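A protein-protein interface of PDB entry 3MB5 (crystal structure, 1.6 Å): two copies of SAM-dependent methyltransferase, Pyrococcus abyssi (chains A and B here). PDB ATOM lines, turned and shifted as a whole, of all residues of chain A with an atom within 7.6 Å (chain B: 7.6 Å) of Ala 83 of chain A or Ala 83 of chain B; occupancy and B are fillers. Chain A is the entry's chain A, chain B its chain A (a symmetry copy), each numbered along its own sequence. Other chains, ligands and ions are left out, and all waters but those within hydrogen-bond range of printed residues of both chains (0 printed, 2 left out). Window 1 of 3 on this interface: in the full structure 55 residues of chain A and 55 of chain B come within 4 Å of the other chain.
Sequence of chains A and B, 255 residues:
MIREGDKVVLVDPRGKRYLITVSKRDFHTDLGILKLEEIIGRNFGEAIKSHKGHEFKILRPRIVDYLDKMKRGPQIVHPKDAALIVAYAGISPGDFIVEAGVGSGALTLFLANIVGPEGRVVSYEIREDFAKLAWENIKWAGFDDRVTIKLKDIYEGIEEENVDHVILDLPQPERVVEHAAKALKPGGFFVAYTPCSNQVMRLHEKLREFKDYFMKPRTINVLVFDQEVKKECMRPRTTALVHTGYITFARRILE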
ATOM      1  N   VAL A  77      16.365  32.591   4.231  1.00  0.00           N
ATOM      2  CA  VAL A  77      16.641  31.467   3.330  1.00  0.00           C
ATOM      3  C   VAL A  77      18.157  31.426   3.113  1.00  0.00           C
ATOM      4  O   VAL A  77      18.775  32.440   2.758  1.00  0.00           O
ATOM      5  CB  VAL A  77      15.889  31.602   1.969  1.00  0.00           C
ATOM      6  CG1 VAL A  77      16.437  30.628   0.936  1.00  0.00           C
ATOM      7  CG2 VAL A  77      14.401  31.360   2.135  1.00  0.00           C
ATOM      8  N   HIS A  78      18.740  30.242   3.331  1.00  0.00           N
ATOM      9  CA  HIS A  78      20.164  29.999   3.203  1.00  0.00           C
ATOM     10  C   HIS A  78      20.590  30.165   1.736  1.00  0.00           C
ATOM     11  O   HIS A  78      19.835  29.778   0.816  1.00  0.00           O
ATOM     12  CB  HIS A  78      20.404  28.562   3.670  1.00  0.00           C
ATOM     13  CG  HIS A  78      21.841  28.208   3.866  1.00  0.00           C
ATOM     14  ND1 HIS A  78      22.688  27.939   2.814  1.00  0.00           N
ATOM     15  CD2 HIS A  78      22.575  28.054   4.994  1.00  0.00           C
ATOM     16  CE1 HIS A  78      23.891  27.654   3.283  1.00  0.00           C
ATOM     17  NE2 HIS A  78      23.847  27.711   4.603  1.00  0.00           N
ATOM     18  N   PRO A  79      21.801  30.702   1.500  1.00  0.00           N
ATOM     19  CA  PRO A  79      22.305  30.854   0.139  1.00  0.00           C
ATOM     20  C   PRO A  79      22.263  29.576  -0.716  1.00  0.00           C
ATOM     21  O   PRO A  79      22.040  29.670  -1.930  1.00  0.00           O
ATOM     22  CB  PRO A  79      23.752  31.334   0.367  1.00  0.00           C
ATOM     23  CG  PRO A  79      23.633  32.164   1.613  1.00  0.00           C
ATOM     24  CD  PRO A  79      22.692  31.368   2.483  1.00  0.00           C
ATOM     25  N   LYS A  80      22.448  28.393  -0.116  1.00  0.00           N
ATOM     26  CA  LYS A  80      22.422  27.149  -0.886  1.00  0.00           C
ATOM     27  C   LYS A  80      21.027  26.918  -1.495  1.00  0.00           C
ATOM     28  O   LYS A  80      20.896  26.361  -2.574  1.00  0.00           O
ATOM     29  CB  LYS A  80      22.847  25.943  -0.020  1.00  0.00           C
ATOM     30  CG  LYS A  80      21.769  25.518   0.960  1.00  0.00           C
ATOM     31  CD  LYS A  80      22.247  24.393   1.895  1.00  0.00           C
ATOM     32  CE  LYS A  80      21.161  24.137   2.930  1.00  0.00           C
ATOM     33  NZ  LYS A  80      19.972  23.468   2.430  1.00  0.00           N
ATOM     34  N   ASP A  81      19.996  27.349  -0.780  1.00  0.00           N
ATOM     35  CA  ASP A  81      18.630  27.136  -1.220  1.00  0.00           C
ATOM     36  C   ASP A  81      18.252  28.201  -2.242  1.00  0.00           C
ATOM     37  O   ASP A  81      17.646  27.847  -3.270  1.00  0.00           O
ATOM     38  CB  ASP A  81      17.700  27.205  -0.002  1.00  0.00           C
ATOM     39  CG  ASP A  81      17.969  26.063   0.989  1.00  0.00           C
ATOM     40  OD1 ASP A  81      18.318  24.951   0.525  1.00  0.00           O
ATOM     41  OD2 ASP A  81      17.841  26.327   2.191  1.00  0.00           O
ATOM     42  N   ALA A  82      18.654  29.437  -1.986  1.00  0.00           N
ATOM     43  CA  ALA A  82      18.469  30.498  -2.989  1.00  0.00           C
ATOM     44  C   ALA A  82      19.176  30.109  -4.294  1.00  0.00           C
ATOM     45  O   ALA A  82      18.646  30.347  -5.403  1.00  0.00           O
ATOM     46  CB  ALA A  82      18.998  31.799  -2.478  1.00  0.00           C
ATOM     47  N   ALA A  83      20.348  29.482  -4.161  1.00  0.00           N
ATOM     48  CA  ALA A  83      21.118  29.096  -5.347  1.00  0.00           C
ATOM     49  C   ALA A  83      20.327  28.119  -6.205  1.00  0.00           C
ATOM     50  O   ALA A  83      20.273  28.248  -7.430  1.00  0.00           O
ATOM     51  CB  ALA A  83      22.430  28.443  -4.944  1.00  0.00           C
ATOM     52  N   LEU A  84      19.699  27.124  -5.564  1.00  0.00           N
ATOM     53  CA  LEU A  84      18.956  26.131  -6.319  1.00  0.00           C
ATOM     54  C   LEU A  84      17.625  26.675  -6.859  1.00  0.00           C
ATOM     55  O   LEU A  84      17.191  26.248  -7.936  1.00  0.00           O
ATOM     56  CB  LEU A  84      18.763  24.841  -5.487  1.00  0.00           C
ATOM     57  CG  LEU A  84      19.817  23.730  -5.733  1.00  0.00           C
ATOM     58  CD1 LEU A  84      19.765  23.228  -7.167  1.00  0.00           C
ATOM     59  CD2 LEU A  84      21.219  24.216  -5.348  1.00  0.00           C
ATOM     60  N   ILE A  85      17.024  27.620  -6.136  1.00  0.00           N
ATOM     61  CA  ILE A  85      15.829  28.312  -6.644  1.00  0.00           C
ATOM     62  C   ILE A  85      16.144  29.032  -7.960  1.00  0.00           C
ATOM     63  O   ILE A  85      15.454  28.835  -8.969  1.00  0.00           O
ATOM     64  CB  ILE A  85      15.251  29.274  -5.609  1.00  0.00           C
ATOM     65  CG1 ILE A  85      14.623  28.487  -4.445  1.00  0.00           C
ATOM     66  CG2 ILE A  85      14.192  30.210  -6.278  1.00  0.00           C
ATOM     67  CD1 ILE A  85      14.304  29.384  -3.221  1.00  0.00           C
ATOM     68  N   VAL A  86      17.239  29.768  -7.957  1.00  0.00           N
ATOM     69  CA  VAL A  86      17.644  30.519  -9.133  1.00  0.00           C
ATOM     70  C   VAL A  86      18.041  29.560 -10.268  1.00  0.00           C
ATOM     71  O   VAL A  86      17.651  29.749 -11.425  1.00  0.00           O
ATOM     72  CB  VAL A  86      18.799  31.517  -8.770  1.00  0.00           C
ATOM     73  CG1 VAL A  86      19.575  31.979 -10.051  1.00  0.00           C
ATOM     74  CG2 VAL A  86      18.215  32.696  -7.986  1.00  0.00           C
ATOM     75  N   ALA A  87      18.786  28.500  -9.929  1.00  0.00           N
ATOM     76  CA  ALA A  87      19.261  27.574 -10.955  1.00  0.00           C
ATOM     77  C   ALA A  87      18.128  26.779 -11.628  1.00  0.00           C
ATOM     78  O   ALA A  87      17.993  26.754 -12.858  1.00  0.00           O
ATOM     79  CB  ALA A  87      20.311  26.631 -10.363  1.00  0.00           C
ATOM     80  N   TYR A  88      17.260  26.168 -10.820  1.00  0.00           N
ATOM     81  CA  TYR A  88      16.301  25.224 -11.373  1.00  0.00           C
ATOM     82  C   TYR A  88      15.057  25.909 -11.947  1.00  0.00           C
ATOM     83  O   TYR A  88      14.381  25.344 -12.809  1.00  0.00           O
ATOM     84  CB  TYR A  88      15.956  24.133 -10.340  1.00  0.00           C
ATOM     85  CG  TYR A  88      17.020  23.064 -10.135  1.00  0.00           C
ATOM     86  CD1 TYR A  88      18.340  23.251 -10.536  1.00  0.00           C
ATOM     87  CD2 TYR A  88      16.688  21.879  -9.498  1.00  0.00           C
ATOM     88  CE1 TYR A  88      19.306  22.258 -10.317  1.00  0.00           C
ATOM     89  CE2 TYR A  88      17.627  20.882  -9.300  1.00  0.00           C
ATOM     90  CZ  TYR A  88      18.926  21.082  -9.709  1.00  0.00           C
ATOM     91  OH  TYR A  88      19.882  20.103  -9.497  1.00  0.00           O
ATOM     92  N   ALA A  89      14.777  27.133 -11.494  1.00  0.00           N
ATOM     93  CA  ALA A  89      13.726  27.929 -12.154  1.00  0.00           C
ATOM     94  C   ALA A  89      14.289  28.808 -13.263  1.00  0.00           C
ATOM     95  O   ALA A  89      13.531  29.528 -13.917  1.00  0.00           O
ATOM     96  CB  ALA A  89      12.945  28.777 -11.135  1.00  0.00           C
ATOM     97  N   LEU A 107      16.453  36.420   0.871  1.00  0.00           N
ATOM     98  CA  LEU A 107      16.116  35.887  -0.437  1.00  0.00           C
ATOM     99  C   LEU A 107      15.871  37.046  -1.426  1.00  0.00           C
ATOM    100  O   LEU A 107      16.275  36.970  -2.575  1.00  0.00           O
ATOM    101  CB  LEU A 107      14.921  34.921  -0.314  1.00  0.00           C
ATOM    102  CG  LEU A 107      14.477  34.281  -1.632  1.00  0.00           C
ATOM    103  CD1 LEU A 107      15.588  33.493  -2.378  1.00  0.00           C
ATOM    104  CD2 LEU A 107      13.287  33.380  -1.339  1.00  0.00           C
ATOM    105  N   PHE A 110      19.150  38.316  -2.749  1.00  0.00           N
ATOM    106  CA  PHE A 110      19.726  37.363  -3.691  1.00  0.00           C
ATOM    107  C   PHE A 110      19.025  37.451  -5.067  1.00  0.00           C
ATOM    108  O   PHE A 110      19.689  37.526  -6.118  1.00  0.00           O
ATOM    109  CB  PHE A 110      19.624  35.966  -3.044  1.00  0.00           C
ATOM    110  CG  PHE A 110      20.456  34.902  -3.710  1.00  0.00           C
ATOM    111  CD1 PHE A 110      21.583  34.391  -3.069  1.00  0.00           C
ATOM    112  CD2 PHE A 110      20.064  34.342  -4.925  1.00  0.00           C
ATOM    113  CE1 PHE A 110      22.339  33.374  -3.669  1.00  0.00           C
ATOM    114  CE2 PHE A 110      20.796  33.332  -5.508  1.00  0.00           C
ATOM    115  CZ  PHE A 110      21.951  32.861  -4.897  1.00  0.00           C
ATOM    116  N   VAL A 222      18.606  20.280  -0.593  1.00  0.00           N
ATOM    117  CA  VAL A 222      20.002  20.495  -0.965  1.00  0.00           C
ATOM    118  C   VAL A 222      20.875  20.427   0.268  1.00  0.00           C
ATOM    119  O   VAL A 222      20.576  21.044   1.301  1.00  0.00           O
ATOM    120  CB  VAL A 222      20.179  21.907  -1.565  1.00  0.00           C
ATOM    121  CG1 VAL A 222      21.634  22.050  -2.125  1.00  0.00           C
ATOM    122  CG2 VAL A 222      19.057  22.208  -2.580  1.00  0.00           C
ATOM    123  N   ILE A 247      12.336  22.376  -1.383  1.00  0.00           N
ATOM    124  CA  ILE A 247      12.039  23.386  -2.402  1.00  0.00           C
ATOM    125  C   ILE A 247      11.220  22.701  -3.476  1.00  0.00           C
ATOM    126  O   ILE A 247      11.646  21.709  -4.080  1.00  0.00           O
ATOM    127  CB  ILE A 247      13.332  23.936  -3.011  1.00  0.00           C
ATOM    128  CG1 ILE A 247      14.284  24.429  -1.925  1.00  0.00           C
ATOM    129  CG2 ILE A 247      12.966  25.144  -3.912  1.00  0.00           C
ATOM    130  CD1 ILE A 247      15.710  24.798  -2.428  1.00  0.00           C
ATOM    131  N   PHE A 249       9.113  23.062  -7.095  1.00  0.00           N
ATOM    132  CA  PHE A 249       9.026  23.823  -8.363  1.00  0.00           C
ATOM    133  C   PHE A 249       7.838  23.313  -9.179  1.00  0.00           C
ATOM    134  O   PHE A 249       7.676  22.128  -9.299  1.00  0.00           O
ATOM    135  CB  PHE A 249      10.291  23.541  -9.213  1.00  0.00           C
ATOM    136  CG  PHE A 249      11.556  24.012  -8.592  1.00  0.00           C
ATOM    137  CD1 PHE A 249      12.225  23.206  -7.651  1.00  0.00           C
ATOM    138  CD2 PHE A 249      12.102  25.245  -8.940  1.00  0.00           C
ATOM    139  CE1 PHE A 249      13.422  23.645  -7.053  1.00  0.00           C
ATOM    140  CE2 PHE A 249      13.306  25.698  -8.359  1.00  0.00           C
ATOM    141  CZ  PHE A 249      13.966  24.903  -7.420  1.00  0.00           C
ATOM    142  N   VAL B  77      29.286  20.437 -16.542  1.00  0.00           N
ATOM    143  CA  VAL B  77      29.077  20.748 -15.124  1.00  0.00           C
ATOM    144  C   VAL B  77      27.565  20.750 -14.882  1.00  0.00           C
ATOM    145  O   VAL B  77      26.807  21.420 -15.599  1.00  0.00           O
ATOM    146  CB  VAL B  77      29.705  22.120 -14.722  1.00  0.00           C
ATOM    147  CG1 VAL B  77      29.199  22.582 -13.363  1.00  0.00           C
ATOM    148  CG2 VAL B  77      31.219  22.043 -14.686  1.00  0.00           C
ATOM    149  N   HIS B  78      27.142  19.992 -13.863  1.00  0.00           N
ATOM    150  CA  HIS B  78      25.750  19.840 -13.484  1.00  0.00           C
ATOM    151  C   HIS B  78      25.200  21.181 -12.977  1.00  0.00           C
ATOM    152  O   HIS B  78      25.925  21.937 -12.292  1.00  0.00           O
ATOM    153  CB  HIS B  78      25.716  18.792 -12.370  1.00  0.00           C
ATOM    154  CG  HIS B  78      24.349  18.299 -12.027  1.00  0.00           C
ATOM    155  ND1 HIS B  78      23.463  19.036 -11.273  1.00  0.00           N
ATOM    156  CD2 HIS B  78      23.724  17.132 -12.314  1.00  0.00           C
ATOM    157  CE1 HIS B  78      22.341  18.354 -11.126  1.00  0.00           C
ATOM    158  NE2 HIS B  78      22.475  17.193 -11.743  1.00  0.00           N
ATOM    159  N   PRO B  79      23.920  21.476 -13.270  1.00  0.00           N
ATOM    160  CA  PRO B  79      23.302  22.707 -12.790  1.00  0.00           C
ATOM    161  C   PRO B  79      23.429  22.950 -11.276  1.00  0.00           C
ATOM    162  O   PRO B  79      23.549  24.110 -10.860  1.00  0.00           O
ATOM    163  CB  PRO B  79      21.830  22.532 -13.212  1.00  0.00           C
ATOM    164  CG  PRO B  79      21.943  21.768 -14.500  1.00  0.00           C
ATOM    165  CD  PRO B  79      23.033  20.762 -14.223  1.00  0.00           C
ATOM    166  N   LYS B  80      23.429  21.895 -10.451  1.00  0.00           N
ATOM    167  CA  LYS B  80      23.543  22.075  -9.004  1.00  0.00           C
ATOM    168  C   LYS B  80      24.907  22.691  -8.640  1.00  0.00           C
ATOM    169  O   LYS B  80      25.021  23.447  -7.688  1.00  0.00           O
ATOM    170  CB  LYS B  80      23.329  20.742  -8.253  1.00  0.00           C
ATOM    171  CG  LYS B  80      24.519  19.808  -8.369  1.00  0.00           C
ATOM    172  CD  LYS B  80      24.247  18.440  -7.717  1.00  0.00           C
ATOM    173  CE  LYS B  80      25.429  17.527  -8.008  1.00  0.00           C
ATOM    174  NZ  LYS B  80      26.648  17.839  -7.281  1.00  0.00           N
ATOM    175  N   ASP B  81      25.930  22.346  -9.410  1.00  0.00           N
ATOM    176  CA  ASP B  81      27.276  22.815  -9.133  1.00  0.00           C
ATOM    177  C   ASP B  81      27.449  24.224  -9.686  1.00  0.00           C
ATOM    178  O   ASP B  81      28.014  25.075  -8.973  1.00  0.00           O
ATOM    179  CB  ASP B  81      28.279  21.854  -9.783  1.00  0.00           C
ATOM    180  CG  ASP B  81      28.220  20.453  -9.156  1.00  0.00           C
ATOM    181  OD1 ASP B  81      27.970  20.368  -7.930  1.00  0.00           O
ATOM    182  OD2 ASP B  81      28.406  19.495  -9.915  1.00  0.00           O
ATOM    183  N   ALA B  82      26.925  24.461 -10.879  1.00  0.00           N
ATOM    184  CA  ALA B  82      26.909  25.829 -11.422  1.00  0.00           C
ATOM    185  C   ALA B  82      26.157  26.760 -10.462  1.00  0.00           C
ATOM    186  O   ALA B  82      26.571  27.922 -10.244  1.00  0.00           O
ATOM    187  CB  ALA B  82      26.271  25.847 -12.773  1.00  0.00           C
ATOM    188  N   ALA B  83      25.080  26.242  -9.866  1.00  0.00           N
ATOM    189  CA  ALA B  83      24.274  27.061  -8.955  1.00  0.00           C
ATOM    190  C   ALA B  83      25.108  27.520  -7.767  1.00  0.00           C
ATOM    191  O   ALA B  83      25.055  28.684  -7.366  1.00  0.00           O
ATOM    192  CB  ALA B  83      23.081  26.271  -8.440  1.00  0.00           C
ATOM    193  N   LEU B  84      25.894  26.601  -7.191  1.00  0.00           N
ATOM    194  CA  LEU B  84      26.690  26.955  -6.029  1.00  0.00           C
ATOM    195  C   LEU B  84      27.904  27.824  -6.389  1.00  0.00           C
ATOM    196  O   LEU B  84      28.304  28.668  -5.578  1.00  0.00           O
ATOM    197  CB  LEU B  84      27.094  25.690  -5.235  1.00  0.00           C
ATOM    198  CG  LEU B  84      26.162  25.326  -4.050  1.00  0.00           C
ATOM    199  CD1 LEU B  84      26.166  26.415  -2.990  1.00  0.00           C
ATOM    200  CD2 LEU B  84      24.746  25.017  -4.548  1.00  0.00           C
ATOM    201  N   ILE B  85      28.443  27.637  -7.593  1.00  0.00           N
ATOM    202  CA  ILE B  85      29.507  28.523  -8.090  1.00  0.00           C
ATOM    203  C   ILE B  85      29.013  29.972  -8.155  1.00  0.00           C
ATOM    204  O   ILE B  85      29.644  30.880  -7.599  1.00  0.00           O
ATOM    205  CB  ILE B  85      30.044  28.058  -9.442  1.00  0.00           C
ATOM    206  CG1 ILE B  85      30.845  26.754  -9.275  1.00  0.00           C
ATOM    207  CG2 ILE B  85      30.934  29.175 -10.079  1.00  0.00           C
ATOM    208  CD1 ILE B  85      31.147  26.062 -10.629  1.00  0.00           C
ATOM    209  N   VAL B  86      27.842  30.147  -8.738  1.00  0.00           N
ATOM    210  CA  VAL B  86      27.266  31.473  -8.884  1.00  0.00           C
ATOM    211  C   VAL B  86      26.900  32.051  -7.506  1.00  0.00           C
ATOM    212  O   VAL B  86      27.178  33.218  -7.213  1.00  0.00           O
ATOM    213  CB  VAL B  86      26.032  31.426  -9.853  1.00  0.00           C
ATOM    214  CG1 VAL B  86      25.114  32.682  -9.666  1.00  0.00           C
ATOM    215  CG2 VAL B  86      26.531  31.279 -11.293  1.00  0.00           C
ATOM    216  N   ALA B  87      26.312  31.217  -6.639  1.00  0.00           N
ATOM    217  CA  ALA B  87      25.873  31.700  -5.332  1.00  0.00           C
ATOM    218  C   ALA B  87      27.038  32.108  -4.413  1.00  0.00           C
ATOM    219  O   ALA B  87      27.083  33.223  -3.876  1.00  0.00           O
ATOM    220  CB  ALA B  87      24.989  30.650  -4.655  1.00  0.00           C
ATOM    221  N   TYR B  88      28.029  31.227  -4.271  1.00  0.00           N
ATOM    222  CA  TYR B  88      29.048  31.445  -3.255  1.00  0.00           C
ATOM    223  C   TYR B  88      30.157  32.393  -3.722  1.00  0.00           C
ATOM    224  O   TYR B  88      30.829  33.014  -2.895  1.00  0.00           O
ATOM    225  CB  TYR B  88      29.595  30.100  -2.739  1.00  0.00           C
ATOM    226  CG  TYR B  88      28.682  29.345  -1.782  1.00  0.00           C
ATOM    227  CD1 TYR B  88      27.323  29.630  -1.682  1.00  0.00           C
ATOM    228  CD2 TYR B  88      29.197  28.316  -1.010  1.00  0.00           C
ATOM    229  CE1 TYR B  88      26.499  28.906  -0.808  1.00  0.00           C
ATOM    230  CE2 TYR B  88      28.398  27.612  -0.126  1.00  0.00           C
ATOM    231  CZ  TYR B  88      27.058  27.913  -0.035  1.00  0.00           C
ATOM    232  OH  TYR B  88      26.242  27.202   0.828  1.00  0.00           O
ATOM    233  N   ALA B  89      30.325  32.528  -5.039  1.00  0.00           N
ATOM    234  CA  ALA B  89      31.223  33.577  -5.554  1.00  0.00           C
ATOM    235  C   ALA B  89      30.481  34.877  -5.832  1.00  0.00           C
ATOM    236  O   ALA B  89      31.098  35.855  -6.259  1.00  0.00           O
ATOM    237  CB  ALA B  89      31.974  33.103  -6.811  1.00  0.00           C
ATOM    238  N   LEU B 107      28.499  25.050 -18.556  1.00  0.00           N
ATOM    239  CA  LEU B 107      28.798  26.048 -17.543  1.00  0.00           C
ATOM    240  C   LEU B 107      28.831  27.450 -18.185  1.00  0.00           C
ATOM    241  O   LEU B 107      28.355  28.407 -17.597  1.00  0.00           O
ATOM    242  CB  LEU B 107      30.104  25.674 -16.814  1.00  0.00           C
ATOM    243  CG  LEU B 107      30.521  26.648 -15.708  1.00  0.00           C
ATOM    244  CD1 LEU B 107      29.457  26.862 -14.597  1.00  0.00           C
ATOM    245  CD2 LEU B 107      31.826  26.148 -15.109  1.00  0.00           C
ATOM    246  N   PHE B 110      25.336  28.788 -18.522  1.00  0.00           N
ATOM    247  CA  PHE B 110      24.808  29.173 -17.219  1.00  0.00           C
ATOM    248  C   PHE B 110      25.389  30.533 -16.764  1.00  0.00           C
ATOM    249  O   PHE B 110      24.645  31.434 -16.334  1.00  0.00           O
ATOM    250  CB  PHE B 110      25.121  28.020 -16.242  1.00  0.00           C
ATOM    251  CG  PHE B 110      24.372  28.080 -14.937  1.00  0.00           C
ATOM    252  CD1 PHE B 110      23.363  27.157 -14.665  1.00  0.00           C
ATOM    253  CD2 PHE B 110      24.734  28.988 -13.944  1.00  0.00           C
ATOM    254  CE1 PHE B 110      22.689  27.186 -13.437  1.00  0.00           C
ATOM    255  CE2 PHE B 110      24.085  29.007 -12.730  1.00  0.00           C
ATOM    256  CZ  PHE B 110      23.042  28.125 -12.479  1.00  0.00           C
ATOM    257  N   VAL B 222      28.148  19.397  -3.220  1.00  0.00           N
ATOM    258  CA  VAL B 222      26.714  19.659  -3.152  1.00  0.00           C
ATOM    259  C   VAL B 222      25.949  18.416  -3.550  1.00  0.00           C
ATOM    260  O   VAL B 222      26.250  17.777  -4.569  1.00  0.00           O
ATOM    261  CB  VAL B 222      26.328  20.766  -4.156  1.00  0.00           C
ATOM    262  CG1 VAL B 222      24.829  21.160  -3.937  1.00  0.00           C
ATOM    263  CG2 VAL B 222      27.328  21.938  -4.078  1.00  0.00           C
ATOM    264  N   ILE B 247      34.054  21.717  -5.240  1.00  0.00           N
ATOM    265  CA  ILE B 247      34.153  23.091  -5.739  1.00  0.00           C
ATOM    266  C   ILE B 247      34.965  23.870  -4.725  1.00  0.00           C
ATOM    267  O   ILE B 247      34.614  23.951  -3.541  1.00  0.00           O
ATOM    268  CB  ILE B 247      32.763  23.718  -5.879  1.00  0.00           C
ATOM    269  CG1 ILE B 247      31.844  22.832  -6.716  1.00  0.00           C
ATOM    270  CG2 ILE B 247      32.917  25.076  -6.612  1.00  0.00           C
ATOM    271  CD1 ILE B 247      30.351  23.272  -6.727  1.00  0.00           C
ATOM    272  N   PHE B 249      36.739  27.530  -3.666  1.00  0.00           N
ATOM    273  CA  PHE B 249      36.642  29.000  -3.818  1.00  0.00           C
ATOM    274  C   PHE B 249      37.817  29.663  -3.099  1.00  0.00           C
ATOM    275  O   PHE B 249      38.108  29.296  -1.992  1.00  0.00           O
ATOM    276  CB  PHE B 249      35.359  29.501  -3.107  1.00  0.00           C
ATOM    277  CG  PHE B 249      34.097  28.989  -3.702  1.00  0.00           C
ATOM    278  CD1 PHE B 249      33.599  27.726  -3.326  1.00  0.00           C
ATOM    279  CD2 PHE B 249      33.386  29.752  -4.624  1.00  0.00           C
ATOM    280  CE1 PHE B 249      32.407  27.230  -3.888  1.00  0.00           C
ATOM    281  CE2 PHE B 249      32.184  29.276  -5.191  1.00  0.00           C
ATOM    282  CZ  PHE B 249      31.694  28.020  -4.825  1.00  0.00           C
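Tyr 88 of chain B touches His 78 of chain A (OH to CE1, 3.4 Å). Lys 80 of chain A touches Tyr 88 of chain B. Ala 83 of chain A touches Ala 83 of chain B (O to CB, 3.6 Å). Ala 83 of chain A touches Ala 87 of chain B. Leu 84 of chain A touches Leu 84 of chain B (CD2 to CD2, 3.7 Å). Ala 83 of chain B touches Ala 87 of chain A. Ala 87 of chain A touches Phe 110 of chain B (CB to CZ, 3.8 Å). Pro 79 of chain B touches Tyr 88 of chain A. Lys 80 of chain B touches Tyr 88 of chain A. Val 222 of chain B touches Val 222 of chain A.
Lys 80 of chain A touches Tyr 88 of chain B, and with the chains exchanged Tyr 88 of chain A touches Lys 80 of chain B. Ala 83 of chain A touches its own counterpart, Ala 83 of chain B. Leu 84 of chain B touches its own counterpart, Leu 84 of chain A. Ala 87 of chain A touches Phe 110 of chain B, and with the chains exchanged Phe 110 of chain A touches Ala 87 of chain B. 18 positions are printed for both chains. Of the 13 pairs that touch across the chains among the printed residues, 13 have their exchanged pair printed and touching as well.
Of the 18 printed residues of chain B, 9 touch a printed residue of chain A. Hydrophobic or aromatic side chains of chain B within 4 Å of the printed part of chain A: His 78, Pro 79, Ala 83, Leu 84, Ala 87, Tyr 88, Phe 110 and Val 222. Printed residues of chain A that touch a printed residue of chain B: His 78, Pro 79, Lys 80, Ala 83, Leu 84, Ala 87, Tyr 88, Phe 110 and Val 222. Hydrophobic or aromatic side chains of chain A that line the printed part of chain B: His 78, Pro 79, Ala 83, Leu 84, Ala 87, Tyr 88, Phe 110 and Val 222. Along chain A the printed residues that touch a printed residue of chain B span positions 78 to 222. Among the printed residues, no Asp or Glu carboxylate lies within 4 Å of a Lys or Arg side-chain nitrogen of the other chain.
Of chain B, only Ala 83 and Ala 87 come within 4 Å of Ala 83 of chain A. Of the printed residues of chain A, Ala 83 of chain B touches Ala 83 and Ala 87. Ala 82 of chain A touches none of the printed residues of chain B. Ala 82 of chain B touches none of the printed residues of chain A. Printed residues of chain B within 4 Å of Ala 87 of chain A: Ala 83 (3.4 Å) and Phe 110 (3.8 Å). Printed residues of chain B within 4 Å of His 78 of chain A: Tyr 88. Printed residues of chain A within 4 Å of Phe 110 of chain B: Ala 87 (3.8 Å). Val 86 of chain B touches none of the printed residues of chain A. The nearest residue of chain A that does not touch Ala 83 of chain B is Leu 84 of chain A (4.2 Å).
A ring nitrogen (ND1) of His 78 of chain A lies within hydrogen-bond range of the backbone NH of Lys 80 of chain A (3.0 Å). NZ of Lys 80 of chain A is in salt-bridge range of OD1 of Asp 81 of chain A, at 2.9 Å. The backbone carbonyl oxygen of Val 222 of chain A sits at hydrogen-bond distance from the side-chain amino group of Lys 80 of chain A, 2.7 Å away. The backbone NH (N) of Lys 80 of chain B is in hydrogen-bond range of a ring nitrogen (ND1) of His 78 of chain B (3.0 Å). The side-chain amino group (NZ) of Lys 80 of chain B is in salt-bridge range of the side-chain carboxylate (OD1) of Asp 81 of chain B (2.9 Å). The side-chain amino group (NZ) of Lys 80 of chain B lies within hydrogen-bond range of the backbone carbonyl oxygen (O) of Val 222 of chain B, 2.7 Å away.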
